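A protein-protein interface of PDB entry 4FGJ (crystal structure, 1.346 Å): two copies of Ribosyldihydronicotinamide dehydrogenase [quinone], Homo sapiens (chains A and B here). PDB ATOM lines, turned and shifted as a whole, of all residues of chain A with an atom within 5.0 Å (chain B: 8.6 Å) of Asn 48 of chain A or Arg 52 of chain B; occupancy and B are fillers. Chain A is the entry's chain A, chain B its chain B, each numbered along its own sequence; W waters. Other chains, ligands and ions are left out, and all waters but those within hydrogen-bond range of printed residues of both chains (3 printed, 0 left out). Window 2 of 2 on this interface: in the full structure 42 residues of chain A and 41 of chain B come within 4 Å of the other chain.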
ATOM      1  N   LEU A  44      23.236   3.748   3.398  1.00  0.00           N
ATOM      2  CA  LEU A  44      21.876   4.217   3.606  1.00  0.00           C
ATOM      3  C   LEU A  44      21.577   5.570   2.969  1.00  0.00           C
ATOM      4  O   LEU A  44      20.531   5.733   2.349  1.00  0.00           O
ATOM      5  CB  LEU A  44      21.568   4.264   5.094  1.00  0.00           C
ATOM      6  CG  LEU A  44      21.666   2.936   5.829  1.00  0.00           C
ATOM      7  CD1 LEU A  44      21.194   3.127   7.267  1.00  0.00           C
ATOM      8  CD2 LEU A  44      20.853   1.862   5.159  1.00  0.00           C
ATOM      9  N   TYR A  45      22.471   6.533   3.069  1.00  0.00           N
ATOM     10  CA  TYR A  45      22.160   7.815   2.448  1.00  0.00           C
ATOM     11  C   TYR A  45      22.100   7.711   0.923  1.00  0.00           C
ATOM     12  O   TYR A  45      21.256   8.332   0.286  1.00  0.00           O
ATOM     13  CB  TYR A  45      23.127   8.908   2.867  1.00  0.00           C
ATOM     14  CG  TYR A  45      22.994   9.382   4.306  1.00  0.00           C
ATOM     15  CD1 TYR A  45      22.003  10.273   4.687  1.00  0.00           C
ATOM     16  CD2 TYR A  45      23.903   8.976   5.266  1.00  0.00           C
ATOM     17  CE1 TYR A  45      21.924  10.726   5.988  1.00  0.00           C
ATOM     18  CE2 TYR A  45      23.834   9.428   6.561  1.00  0.00           C
ATOM     19  CZ  TYR A  45      22.846  10.308   6.928  1.00  0.00           C
ATOM     20  OH  TYR A  45      22.780  10.759   8.229  1.00  0.00           O
ATOM     21  N   ALA A  46      23.016   6.947   0.337  1.00  0.00           N
ATOM     22  CA  ALA A  46      23.038   6.779  -1.130  1.00  0.00           C
ATOM     23  C   ALA A  46      21.775   6.066  -1.622  1.00  0.00           C
ATOM     24  O   ALA A  46      21.280   6.313  -2.729  1.00  0.00           O
ATOM     25  CB  ALA A  46      24.280   6.019  -1.563  1.00  0.00           C
ATOM     26  N   MET A  47      21.263   5.169  -0.787  1.00  0.00           N
ATOM     27  CA  MET A  47      20.014   4.445  -1.045  1.00  0.00           C
ATOM     28  C   MET A  47      18.775   5.284  -0.771  1.00  0.00           C
ATOM     29  O   MET A  47      17.665   4.854  -1.054  1.00  0.00           O
ATOM     30  CB  MET A  47      19.946   3.207  -0.150  1.00  0.00           C
ATOM     31  CG  MET A  47      21.044   2.177  -0.413  1.00  0.00           C
ATOM     32  SD  MET A  47      21.233   1.008   0.948  1.00  0.00           S
ATOM     33  CE  MET A  47      19.674   0.143   0.817  1.00  0.00           C
ATOM     34  N   ASN A  48      18.968   6.484  -0.234  1.00  0.00           N
ATOM     35  CA  ASN A  48      17.861   7.302   0.254  1.00  0.00           C
ATOM     36  C   ASN A  48      16.912   6.489   1.143  1.00  0.00           C
ATOM     37  O   ASN A  48      15.685   6.557   1.028  1.00  0.00           O
ATOM     38  CB  ASN A  48      17.086   7.963  -0.880  1.00  0.00           C
ATOM     39  CG  ASN A  48      16.281   9.144  -0.391  1.00  0.00           C
ATOM     40  OD1 ASN A  48      16.719   9.893   0.500  1.00  0.00           O
ATOM     41  ND2 ASN A  48      15.087   9.294  -0.931  1.00  0.00           N
ATOM     42  N   PHE A  49      17.515   5.710   2.034  1.00  0.00           N
ATOM     43  CA  PHE A  49      16.794   4.749   2.836  1.00  0.00           C
ATOM     44  C   PHE A  49      15.703   5.451   3.638  1.00  0.00           C
ATOM     45  O   PHE A  49      15.952   6.474   4.298  1.00  0.00           O
ATOM     46  CB  PHE A  49      17.737   3.985   3.771  1.00  0.00           C
ATOM     47  CG  PHE A  49      17.069   2.854   4.454  1.00  0.00           C
ATOM     48  CD1 PHE A  49      16.927   1.636   3.805  1.00  0.00           C
ATOM     49  CD2 PHE A  49      16.555   2.992   5.734  1.00  0.00           C
ATOM     50  CE1 PHE A  49      16.278   0.584   4.416  1.00  0.00           C
ATOM     51  CE2 PHE A  49      15.902   1.952   6.344  1.00  0.00           C
ATOM     52  CZ  PHE A  49      15.755   0.753   5.698  1.00  0.00           C
ATOM     53  N   GLU A  50      14.494   4.897   3.570  1.00  0.00           N
ATOM     54  CA  GLU A  50      13.333   5.450   4.283  1.00  0.00           C
ATOM     55  C   GLU A  50      13.436   5.183   5.787  1.00  0.00           C
ATOM     56  O   GLU A  50      13.464   4.030   6.196  1.00  0.00           O
ATOM     57  CB  GLU A  50      12.055   4.794   3.770  1.00  0.00           C
ATOM     58  CG  GLU A  50      10.818   5.158   4.566  1.00  0.00           C
ATOM     59  CD  GLU A  50      10.495   6.643   4.490  1.00  0.00           C
ATOM     60  OE1 GLU A  50      10.144   7.119   3.387  1.00  0.00           O
ATOM     61  OE2 GLU A  50      10.602   7.334   5.522  1.00  0.00           O
ATOM     62  N   PRO A  51      13.464   6.240   6.621  1.00  0.00           N
ATOM     63  CA  PRO A  51      13.568   5.986   8.060  1.00  0.00           C
ATOM     64  C   PRO A  51      12.244   5.857   8.780  1.00  0.00           C
ATOM     65  O   PRO A  51      12.231   5.343   9.898  1.00  0.00           O
ATOM     66  CB  PRO A  51      14.324   7.224   8.600  1.00  0.00           C
ATOM     67  CG  PRO A  51      14.749   7.993   7.396  1.00  0.00           C
ATOM     68  CD  PRO A  51      13.794   7.632   6.306  1.00  0.00           C
ATOM     69  N   ARG A  52      11.162   6.345   8.181  1.00  0.00           N
ATOM     70  CA  ARG A  52       9.909   6.434   8.902  1.00  0.00           C
ATOM     71  C   ARG A  52       9.177   5.100   8.928  1.00  0.00           C
ATOM     72  O   ARG A  52       9.040   4.441   7.903  1.00  0.00           O
ATOM     73  CB  ARG A  52       8.991   7.477   8.248  1.00  0.00           C
ATOM     74  CG  ARG A  52       9.575   8.901   8.126  1.00  0.00           C
ATOM     75  CD  ARG A  52       8.601   9.686   7.285  1.00  0.00           C
ATOM     76  NE  ARG A  52       9.026  10.986   6.768  1.00  0.00           N
ATOM     77  CZ  ARG A  52       9.639  11.180   5.600  1.00  0.00           C
ATOM     78  NH1 ARG A  52      10.025  10.168   4.827  1.00  0.00           N
ATOM     79  NH2 ARG A  52       9.915  12.408   5.210  1.00  0.00           N
ATOM     80  N   ILE A 114      18.696   8.112   9.995  1.00  0.00           N
ATOM     81  CA  ILE A 114      18.521   7.209   8.876  1.00  0.00           C
ATOM     82  C   ILE A 114      18.841   5.776   9.293  1.00  0.00           C
ATOM     83  O   ILE A 114      18.165   4.832   8.862  1.00  0.00           O
ATOM     84  CB  ILE A 114      19.316   7.682   7.643  1.00  0.00           C
ATOM     85  CG1 ILE A 114      18.822   6.969   6.385  1.00  0.00           C
ATOM     86  CG2 ILE A 114      20.827   7.486   7.819  1.00  0.00           C
ATOM     87  CD1 ILE A 114      19.373   7.573   5.099  1.00  0.00           C
ATOM     88  N   ASN B  48       4.712  14.337   7.689  1.00  0.00           N
ATOM     89  CA  ASN B  48       5.724  13.647   6.874  1.00  0.00           C
ATOM     90  C   ASN B  48       7.111  14.223   7.119  1.00  0.00           C
ATOM     91  O   ASN B  48       7.904  14.399   6.203  1.00  0.00           O
ATOM     92  CB  ASN B  48       5.394  13.694   5.376  1.00  0.00           C
ATOM     93  CG  ASN B  48       6.169  12.658   4.604  1.00  0.00           C
ATOM     94  OD1 ASN B  48       6.398  11.558   5.111  1.00  0.00           O
ATOM     95  ND2 ASN B  48       6.603  12.999   3.395  1.00  0.00           N
ATOM     96  N   PHE B  49       7.409  14.489   8.383  1.00  0.00           N
ATOM     97  CA  PHE B  49       8.644  15.158   8.756  1.00  0.00           C
ATOM     98  C   PHE B  49       9.855  14.403   8.243  1.00  0.00           C
ATOM     99  O   PHE B  49       9.961  13.183   8.410  1.00  0.00           O
ATOM    100  CB  PHE B  49       8.731  15.310  10.270  1.00  0.00           C
ATOM    101  CG  PHE B  49       9.859  16.168  10.687  1.00  0.00           C
ATOM    102  CD1 PHE B  49       9.731  17.549  10.663  1.00  0.00           C
ATOM    103  CD2 PHE B  49      11.068  15.619  11.059  1.00  0.00           C
ATOM    104  CE1 PHE B  49      10.800  18.353  11.016  1.00  0.00           C
ATOM    105  CE2 PHE B  49      12.122  16.409  11.410  1.00  0.00           C
ATOM    106  CZ  PHE B  49      12.000  17.776  11.377  1.00  0.00           C
ATOM    107  N   GLU B  50      10.758  15.134   7.592  1.00  0.00           N
ATOM    108  CA  GLU B  50      11.969  14.540   7.010  1.00  0.00           C
ATOM    109  C   GLU B  50      12.976  14.190   8.109  1.00  0.00           C
ATOM    110  O   GLU B  50      13.439  15.065   8.808  1.00  0.00           O
ATOM    111  CB  GLU B  50      12.627  15.570   6.094  1.00  0.00           C
ATOM    112  CG  GLU B  50      13.988  15.131   5.559  1.00  0.00           C
ATOM    113  CD  GLU B  50      13.911  13.849   4.758  1.00  0.00           C
ATOM    114  OE1 GLU B  50      13.280  13.854   3.677  1.00  0.00           O
ATOM    115  OE2 GLU B  50      14.474  12.831   5.208  1.00  0.00           O
ATOM    116  N   PRO B  51      13.354  12.909   8.245  1.00  0.00           N
ATOM    117  CA  PRO B  51      14.306  12.562   9.319  1.00  0.00           C
ATOM    118  C   PRO B  51      15.769  12.588   8.907  1.00  0.00           C
ATOM    119  O   PRO B  51      16.642  12.608   9.769  1.00  0.00           O
ATOM    120  CB  PRO B  51      13.923  11.111   9.670  1.00  0.00           C
ATOM    121  CG  PRO B  51      12.665  10.821   8.927  1.00  0.00           C
ATOM    122  CD  PRO B  51      12.697  11.706   7.719  1.00  0.00           C
ATOM    123  N   ARG B  52      16.042  12.536   7.609  1.00  0.00           N
ATOM    124  CA  ARG B  52      17.414  12.348   7.156  1.00  0.00           C
ATOM    125  C   ARG B  52      18.205  13.652   7.187  1.00  0.00           C
ATOM    126  O   ARG B  52      17.721  14.677   6.705  1.00  0.00           O
ATOM    127  CB  ARG B  52      17.436  11.821   5.729  1.00  0.00           C
ATOM    128  CG  ARG B  52      16.663  10.512   5.489  1.00  0.00           C
ATOM    129  CD  ARG B  52      16.662  10.248   3.995  1.00  0.00           C
ATOM    130  NE  ARG B  52      15.772   9.220   3.476  1.00  0.00           N
ATOM    131  CZ  ARG B  52      14.500   9.405   3.106  1.00  0.00           C
ATOM    132  NH1 ARG B  52      13.863  10.568   3.266  1.00  0.00           N
ATOM    133  NH2 ARG B  52      13.844   8.394   2.583  1.00  0.00           N
ATOM    134  N   ALA B  53      19.422  13.599   7.725  1.00  0.00           N
ATOM    135  CA  ALA B  53      20.337  14.733   7.713  1.00  0.00           C
ATOM    136  C   ALA B  53      21.054  14.731   6.371  1.00  0.00           C
ATOM    137  O   ALA B  53      21.937  13.899   6.140  1.00  0.00           O
ATOM    138  CB  ALA B  53      21.336  14.614   8.848  1.00  0.00           C
ATOM    139  N   THR B  54      20.662  15.613   5.458  1.00  0.00           N
ATOM    140  CA  THR B  54      21.260  15.627   4.122  1.00  0.00           C
ATOM    141  C   THR B  54      21.617  17.031   3.661  1.00  0.00           C
ATOM    142  O   THR B  54      21.228  18.015   4.280  1.00  0.00           O
ATOM    143  CB  THR B  54      20.358  15.004   3.034  1.00  0.00           C
ATOM    144  OG1 THR B  54      19.340  15.938   2.645  1.00  0.00           O
ATOM    145  CG2 THR B  54      19.755  13.693   3.488  1.00  0.00           C
ATOM    146  N   ASP B  55      22.319  17.119   2.539  1.00  0.00           N
ATOM    147  CA  ASP B  55      22.701  18.406   1.997  1.00  0.00           C
ATOM    148  C   ASP B  55      21.497  19.202   1.493  1.00  0.00           C
ATOM    149  O   ASP B  55      21.624  20.383   1.206  1.00  0.00           O
ATOM    150  CB  ASP B  55      23.804  18.269   0.928  1.00  0.00           C
ATOM    151  CG  ASP B  55      23.389  17.440  -0.271  1.00  0.00           C
ATOM    152  OD1 ASP B  55      22.199  17.160  -0.474  1.00  0.00           O
ATOM    153  OD2 ASP B  55      24.305  17.064  -1.037  1.00  0.00           O
ATOM    154  N   LYS B  56      20.324  18.581   1.417  1.00  0.00           N
ATOM    155  CA  LYS B  56      19.110  19.348   1.101  1.00  0.00           C
ATOM    156  C   LYS B  56      18.685  20.266   2.251  1.00  0.00           C
ATOM    157  O   LYS B  56      17.782  21.094   2.091  1.00  0.00           O
ATOM    158  CB  LYS B  56      17.955  18.403   0.749  1.00  0.00           C
ATOM    159  CG  LYS B  56      18.197  17.542  -0.495  1.00  0.00           C
ATOM    160  CD  LYS B  56      18.566  18.394  -1.698  1.00  0.00           C
ATOM    161  CE  LYS B  56      18.721  17.570  -2.965  1.00  0.00           C
ATOM    162  NZ  LYS B  56      19.267  18.398  -4.079  1.00  0.00           N
ATOM    163  N   ASP B  57      19.324  20.115   3.408  1.00  0.00           N
ATOM    164  CA  ASP B  57      18.977  20.909   4.575  1.00  0.00           C
ATOM    165  C   ASP B  57      19.634  22.274   4.525  1.00  0.00           C
ATOM    166  O   ASP B  57      19.328  23.136   5.344  1.00  0.00           O
ATOM    167  CB  ASP B  57      19.370  20.173   5.859  1.00  0.00           C
ATOM    168  CG  ASP B  57      18.530  18.930   6.086  1.00  0.00           C
ATOM    169  OD1 ASP B  57      17.519  18.775   5.353  1.00  0.00           O
ATOM    170  OD2 ASP B  57      18.867  18.125   6.988  1.00  0.00           O
ATOM    171  N   TYR B  70      27.994  17.687   7.632  1.00  0.00           N
ATOM    172  CA  TYR B  70      26.656  18.128   8.007  1.00  0.00           C
ATOM    173  C   TYR B  70      26.687  19.129   9.157  1.00  0.00           C
ATOM    174  O   TYR B  70      26.000  20.155   9.115  1.00  0.00           O
ATOM    175  CB  TYR B  70      25.761  16.922   8.339  1.00  0.00           C
ATOM    176  CG  TYR B  70      24.318  17.322   8.551  1.00  0.00           C
ATOM    177  CD1 TYR B  70      23.478  17.538   7.464  1.00  0.00           C
ATOM    178  CD2 TYR B  70      23.795  17.498   9.828  1.00  0.00           C
ATOM    179  CE1 TYR B  70      22.163  17.937   7.639  1.00  0.00           C
ATOM    180  CE2 TYR B  70      22.476  17.884  10.010  1.00  0.00           C
ATOM    181  CZ  TYR B  70      21.668  18.110   8.924  1.00  0.00           C
ATOM    182  OH  TYR B  70      20.363  18.494   9.107  1.00  0.00           O
ATOM    183  N   ASP B  86      11.659  23.732   6.794  1.00  0.00           N
ATOM    184  CA  ASP B  86      11.047  22.823   7.761  1.00  0.00           C
ATOM    185  C   ASP B  86      11.804  22.831   9.083  1.00  0.00           C
ATOM    186  O   ASP B  86      11.200  22.721  10.153  1.00  0.00           O
ATOM    187  CB  ASP B  86      10.857  21.391   7.208  1.00  0.00           C
ATOM    188  CG  ASP B  86      12.156  20.656   6.885  1.00  0.00           C
ATOM    189  OD1 ASP B  86      13.183  21.272   6.555  1.00  0.00           O
ATOM    190  OD2 ASP B  86      12.130  19.407   6.912  1.00  0.00           O
ATOM    191  N   ILE B  87      13.120  22.986   9.007  1.00  0.00           N
ATOM    192  CA  ILE B  87      13.944  23.080  10.201  1.00  0.00           C
ATOM    193  C   ILE B  87      13.656  24.379  10.943  1.00  0.00           C
ATOM    194  O   ILE B  87      13.394  24.373  12.141  1.00  0.00           O
ATOM    195  CB  ILE B  87      15.433  22.993   9.835  1.00  0.00           C
ATOM    196  CG1 ILE B  87      15.748  21.573   9.341  1.00  0.00           C
ATOM    197  CG2 ILE B  87      16.280  23.366  11.031  1.00  0.00           C
ATOM    198  CD1 ILE B  87      17.103  21.441   8.694  1.00  0.00           C
ATOM    199  N   ALA B 113      12.565   6.736  14.736  1.00  0.00           N
ATOM    200  CA  ALA B 113      13.470   7.448  13.838  1.00  0.00           C
ATOM    201  C   ALA B 113      12.958   8.810  13.376  1.00  0.00           C
ATOM    202  O   ALA B 113      13.741   9.736  13.164  1.00  0.00           O
ATOM    203  CB  ALA B 113      13.822   6.577  12.628  1.00  0.00           C
ATOM    204  N   ILE B 114      11.656   8.960  13.186  1.00  0.00           N
ATOM    205  CA  ILE B 114      11.167  10.241  12.704  1.00  0.00           C
ATOM    206  C   ILE B 114      11.435  11.347  13.733  1.00  0.00           C
ATOM    207  O   ILE B 114      11.762  12.470  13.378  1.00  0.00           O
ATOM    208  CB  ILE B 114       9.663  10.163  12.313  1.00  0.00           C
ATOM    209  CG1 ILE B 114       9.271  11.379  11.498  1.00  0.00           C
ATOM    210  CG2 ILE B 114       8.749   9.954  13.521  1.00  0.00           C
ATOM    211  CD1 ILE B 114       7.865  11.261  10.882  1.00  0.00           C
ATOM    212  N   LYS B 116      13.902  10.985  16.127  1.00  0.00           N
ATOM    213  CA  LYS B 116      15.357  11.123  16.144  1.00  0.00           C
ATOM    214  C   LYS B 116      15.788  12.145  15.088  1.00  0.00           C
ATOM    215  O   LYS B 116      16.693  12.939  15.301  1.00  0.00           O
ATOM    216  CB  LYS B 116      16.053   9.781  15.893  1.00  0.00           C
ATOM    217  CG  LYS B 116      17.569   9.859  16.012  1.00  0.00           C
ATOM    218  CD  LYS B 116      18.012  10.503  17.326  1.00  0.00           C
ATOM    219  CE  LYS B 116      19.435  10.179  17.710  1.00  0.00           C
ATOM    220  NZ  LYS B 116      20.387  10.596  16.655  1.00  0.00           N
ATOM    221  N   GLY B 117      15.146  12.123  13.925  1.00  0.00           N
ATOM    222  CA  GLY B 117      15.489  13.059  12.872  1.00  0.00           C
ATOM    223  C   GLY B 117      15.165  14.496  13.207  1.00  0.00           C
ATOM    224  O   GLY B 117      15.869  15.417  12.807  1.00  0.00           O
ATOM    225  N   TRP B 118      14.076  14.692  13.936  1.00  0.00           N
ATOM    226  CA  TRP B 118      13.744  16.013  14.458  1.00  0.00           C
ATOM    227  C   TRP B 118      14.892  16.494  15.358  1.00  0.00           C
ATOM    228  O   TRP B 118      15.355  17.619  15.236  1.00  0.00           O
ATOM    229  CB  TRP B 118      12.394  15.964  15.196  1.00  0.00           C
ATOM    230  CG  TRP B 118      11.852  17.284  15.662  1.00  0.00           C
ATOM    231  CD1 TRP B 118      10.885  18.029  15.051  1.00  0.00           C
ATOM    232  CD2 TRP B 118      12.206  17.993  16.855  1.00  0.00           C
ATOM    233  NE1 TRP B 118      10.617  19.154  15.785  1.00  0.00           N
ATOM    234  CE2 TRP B 118      11.415  19.156  16.901  1.00  0.00           C
ATOM    235  CE3 TRP B 118      13.116  17.758  17.891  1.00  0.00           C
ATOM    236  CZ2 TRP B 118      11.524  20.096  17.938  1.00  0.00           C
ATOM    237  CZ3 TRP B 118      13.207  18.674  18.916  1.00  0.00           C
ATOM    238  CH2 TRP B 118      12.427  19.837  18.927  1.00  0.00           C
ATOM    239  N   ASP B 120      18.029  15.476  15.359  1.00  0.00           N
ATOM    240  CA  ASP B 120      19.235  15.623  14.578  1.00  0.00           C
ATOM    241  C   ASP B 120      19.241  16.917  13.772  1.00  0.00           C
ATOM    242  O   ASP B 120      20.273  17.583  13.664  1.00  0.00           O
ATOM    243  CB  ASP B 120      19.386  14.473  13.587  1.00  0.00           C
ATOM    244  CG  ASP B 120      19.625  13.109  14.226  1.00  0.00           C
ATOM    245  OD1 ASP B 120      19.938  13.018  15.443  1.00  0.00           O
ATOM    246  OD2 ASP B 120      19.525  12.104  13.457  1.00  0.00           O
ATOM    247  N   ARG B 121      18.101  17.235  13.156  1.00  0.00           N
ATOM    248  CA  ARG B 121      18.021  18.328  12.193  1.00  0.00           C
ATOM    249  C   ARG B 121      17.661  19.667  12.828  1.00  0.00           C
ATOM    250  O   ARG B 121      18.082  20.714  12.347  1.00  0.00           O
ATOM    251  CB  ARG B 121      17.021  17.990  11.093  1.00  0.00           C
ATOM    252  CG  ARG B 121      17.412  16.774  10.270  1.00  0.00           C
ATOM    253  CD  ARG B 121      16.331  16.376   9.261  1.00  0.00           C
ATOM    254  NE  ARG B 121      16.220  17.339   8.169  1.00  0.00           N
ATOM    255  CZ  ARG B 121      15.137  18.072   7.905  1.00  0.00           C
ATOM    256  NH1 ARG B 121      14.016  17.925   8.602  1.00  0.00           N
ATOM    257  NH2 ARG B 121      15.149  18.953   6.920  1.00  0.00           N
HETATM  258  O   HOH W   1      11.102   9.199   2.180  1.00  0.00           O
HETATM  259  O   HOH W   2      11.473  12.217   2.743  1.00  0.00           O
HETATM  260  O   HOH W   3      20.066  10.628   9.188  1.00  0.00           O
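The backbone carbonyl oxygen of Asn 48 of chain A lies within hydrogen-bond range of the guanidinium group of Arg 52 of chain B, at 3.0 Å. The backbone carbonyl oxygen (O) of Phe 49 of chain A lies within hydrogen-bond range of the guanidinium group (NE) of Arg 52 of chain B (2.9 Å). NH2 of Arg 52 of chain B is in salt-bridge range of OE1 of Glu 50 of chain A. NH2 of Arg 52 of chain A lies within hydrogen-bond range of O of Asn 48 of chain B (3.0 Å). The backbone carbonyl oxygen (O) of Phe 49 of chain B lies within hydrogen-bond range of the guanidinium group (NE) of Arg 52 of chain A, at 2.9 Å. NH2 of Arg 52 of chain A lies within salt-bridge range of OE1 of Glu 50 of chain B, 3.97 Å away.
The backbone NH (N) of Phe 49 of chain A sits at hydrogen-bond distance from the backbone carbonyl oxygen (O) of Leu 44 of chain A (3.0 Å). The side-chain carboxylate (OE2) of Glu 50 of chain A is in salt-bridge range of the guanidinium group (NH1) of Arg 52 of chain A, 3.0 Å away. The side-chain carboxylate (OE2) of Glu 50 of chain B lies within salt-bridge range of the guanidinium group (NH1) of Arg 52 of chain B, at 3.0 Å. O of Glu 50 of chain B is in hydrogen-bond range of NH1 of Arg 121 of chain B, 2.9 Å away. The backbone carbonyl oxygen (O) of Arg 52 of chain B lies close to the guanidinium group (NE) of Arg 121 of chain B, 3.4 Å away.
Ala 53 of chain B touches Tyr 45 of chain A (O to CE1, 3.2 Å). Pro 51 of chain B touches Pro 51 of chain A. Pro 51 of chain A touches Arg 52 of chain B. CB of Ala 113 of chain B touches O of Pro 51 of chain A, 3.4 Å away. CG of Pro 51 of chain B touches CG of Arg 52 of chain A (3.7 Å). CD1 of Ile 114 of chain B touches CD of Arg 52 of chain A, at 3.995 Å. CD of Arg 52 of chain B touches CD1 of Ile 114 of chain A, 3.97 Å away.
Of the printed residues of chain B, Asn 48 of chain A touches Arg 52 (3.0 Å). Arg 52 of chain B touches five residues of chain A. Of the printed residues of chain A, Ile 114 of chain B touches Arg 52. Printed residues of chain B within 4 Å of Phe 49 of chain A: Arg 52. Of the printed residues of chain A, Ala 53 of chain B touches Tyr 45. Printed residues of chain B within 4 Å of Glu 50 of chain A: Arg 52 (3.4 Å). Of the printed residues of chain A, Phe 49 of chain B touches Arg 52 (2.9 Å). Thr 54 of chain B touches none of the printed residues of chain A. The nearest residue of chain B that does not touch Asn 48 of chain A is Thr 54 of chain B (5.7 Å). The nearest residue of chain A that does not touch Arg 52 of chain B is Arg 52 of chain A (4.2 Å).
Printed residues of chain A that touch a printed residue of chain B: Tyr 45, Asn 48, Phe 49, Glu 50, Pro 51, Arg 52 and Ile 114. Hydrophobic or aromatic side chains of chain A within 4 Å of the printed part of chain B: Tyr 45, Pro 51 and Ile 114. Of the 20 printed residues of chain B, 8 touch a printed residue of chain A. Among the printed residues, 13 pairs touch across the chains.
Asn 48 of chain A touches Arg 52 of chain B, and with the chains exchanged Arg 52 of chain A touches Asn 48 of chain B. Glu 50 of chain A touches Arg 52 of chain B, and with the chains exchanged Arg 52 of chain A touches Glu 50 of chain B. Pro 51 of chain A touches Arg 52 of chain B, and with the chains exchanged Arg 52 of chain A touches Pro 51 of chain B. Arg 52 of chain A touches Ile 114 of chain B, and with the chains exchanged Ile 114 of chain A touches Arg 52 of chain B. Positions printed for both chains: 48, 49, 50, 51, 52 and 114.
Water W1 lies within hydrogen-bond range of the side-chain carboxylate (OE1) of Glu 50 of chain A, the guanidinium group (NH2) of Arg 52 of chain B and the guanidinium group (NH1) of Arg 52 of chain A. Water W2 lies within hydrogen-bond range of OE1 of Glu 50 of chain B (2.6 Å), NH2 of Arg 52 of chain A (2.9 Å) and NH1 of Arg 52 of chain B (3.0 Å). Water W3 lies within hydrogen-bond range of the side-chain hydroxyl of Tyr 45 of chain A (2.9 Å), the backbone NH of Ile 114 of chain A (3.0 Å) and the backbone NH of Ala 53 of chain B (3.4 Å).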
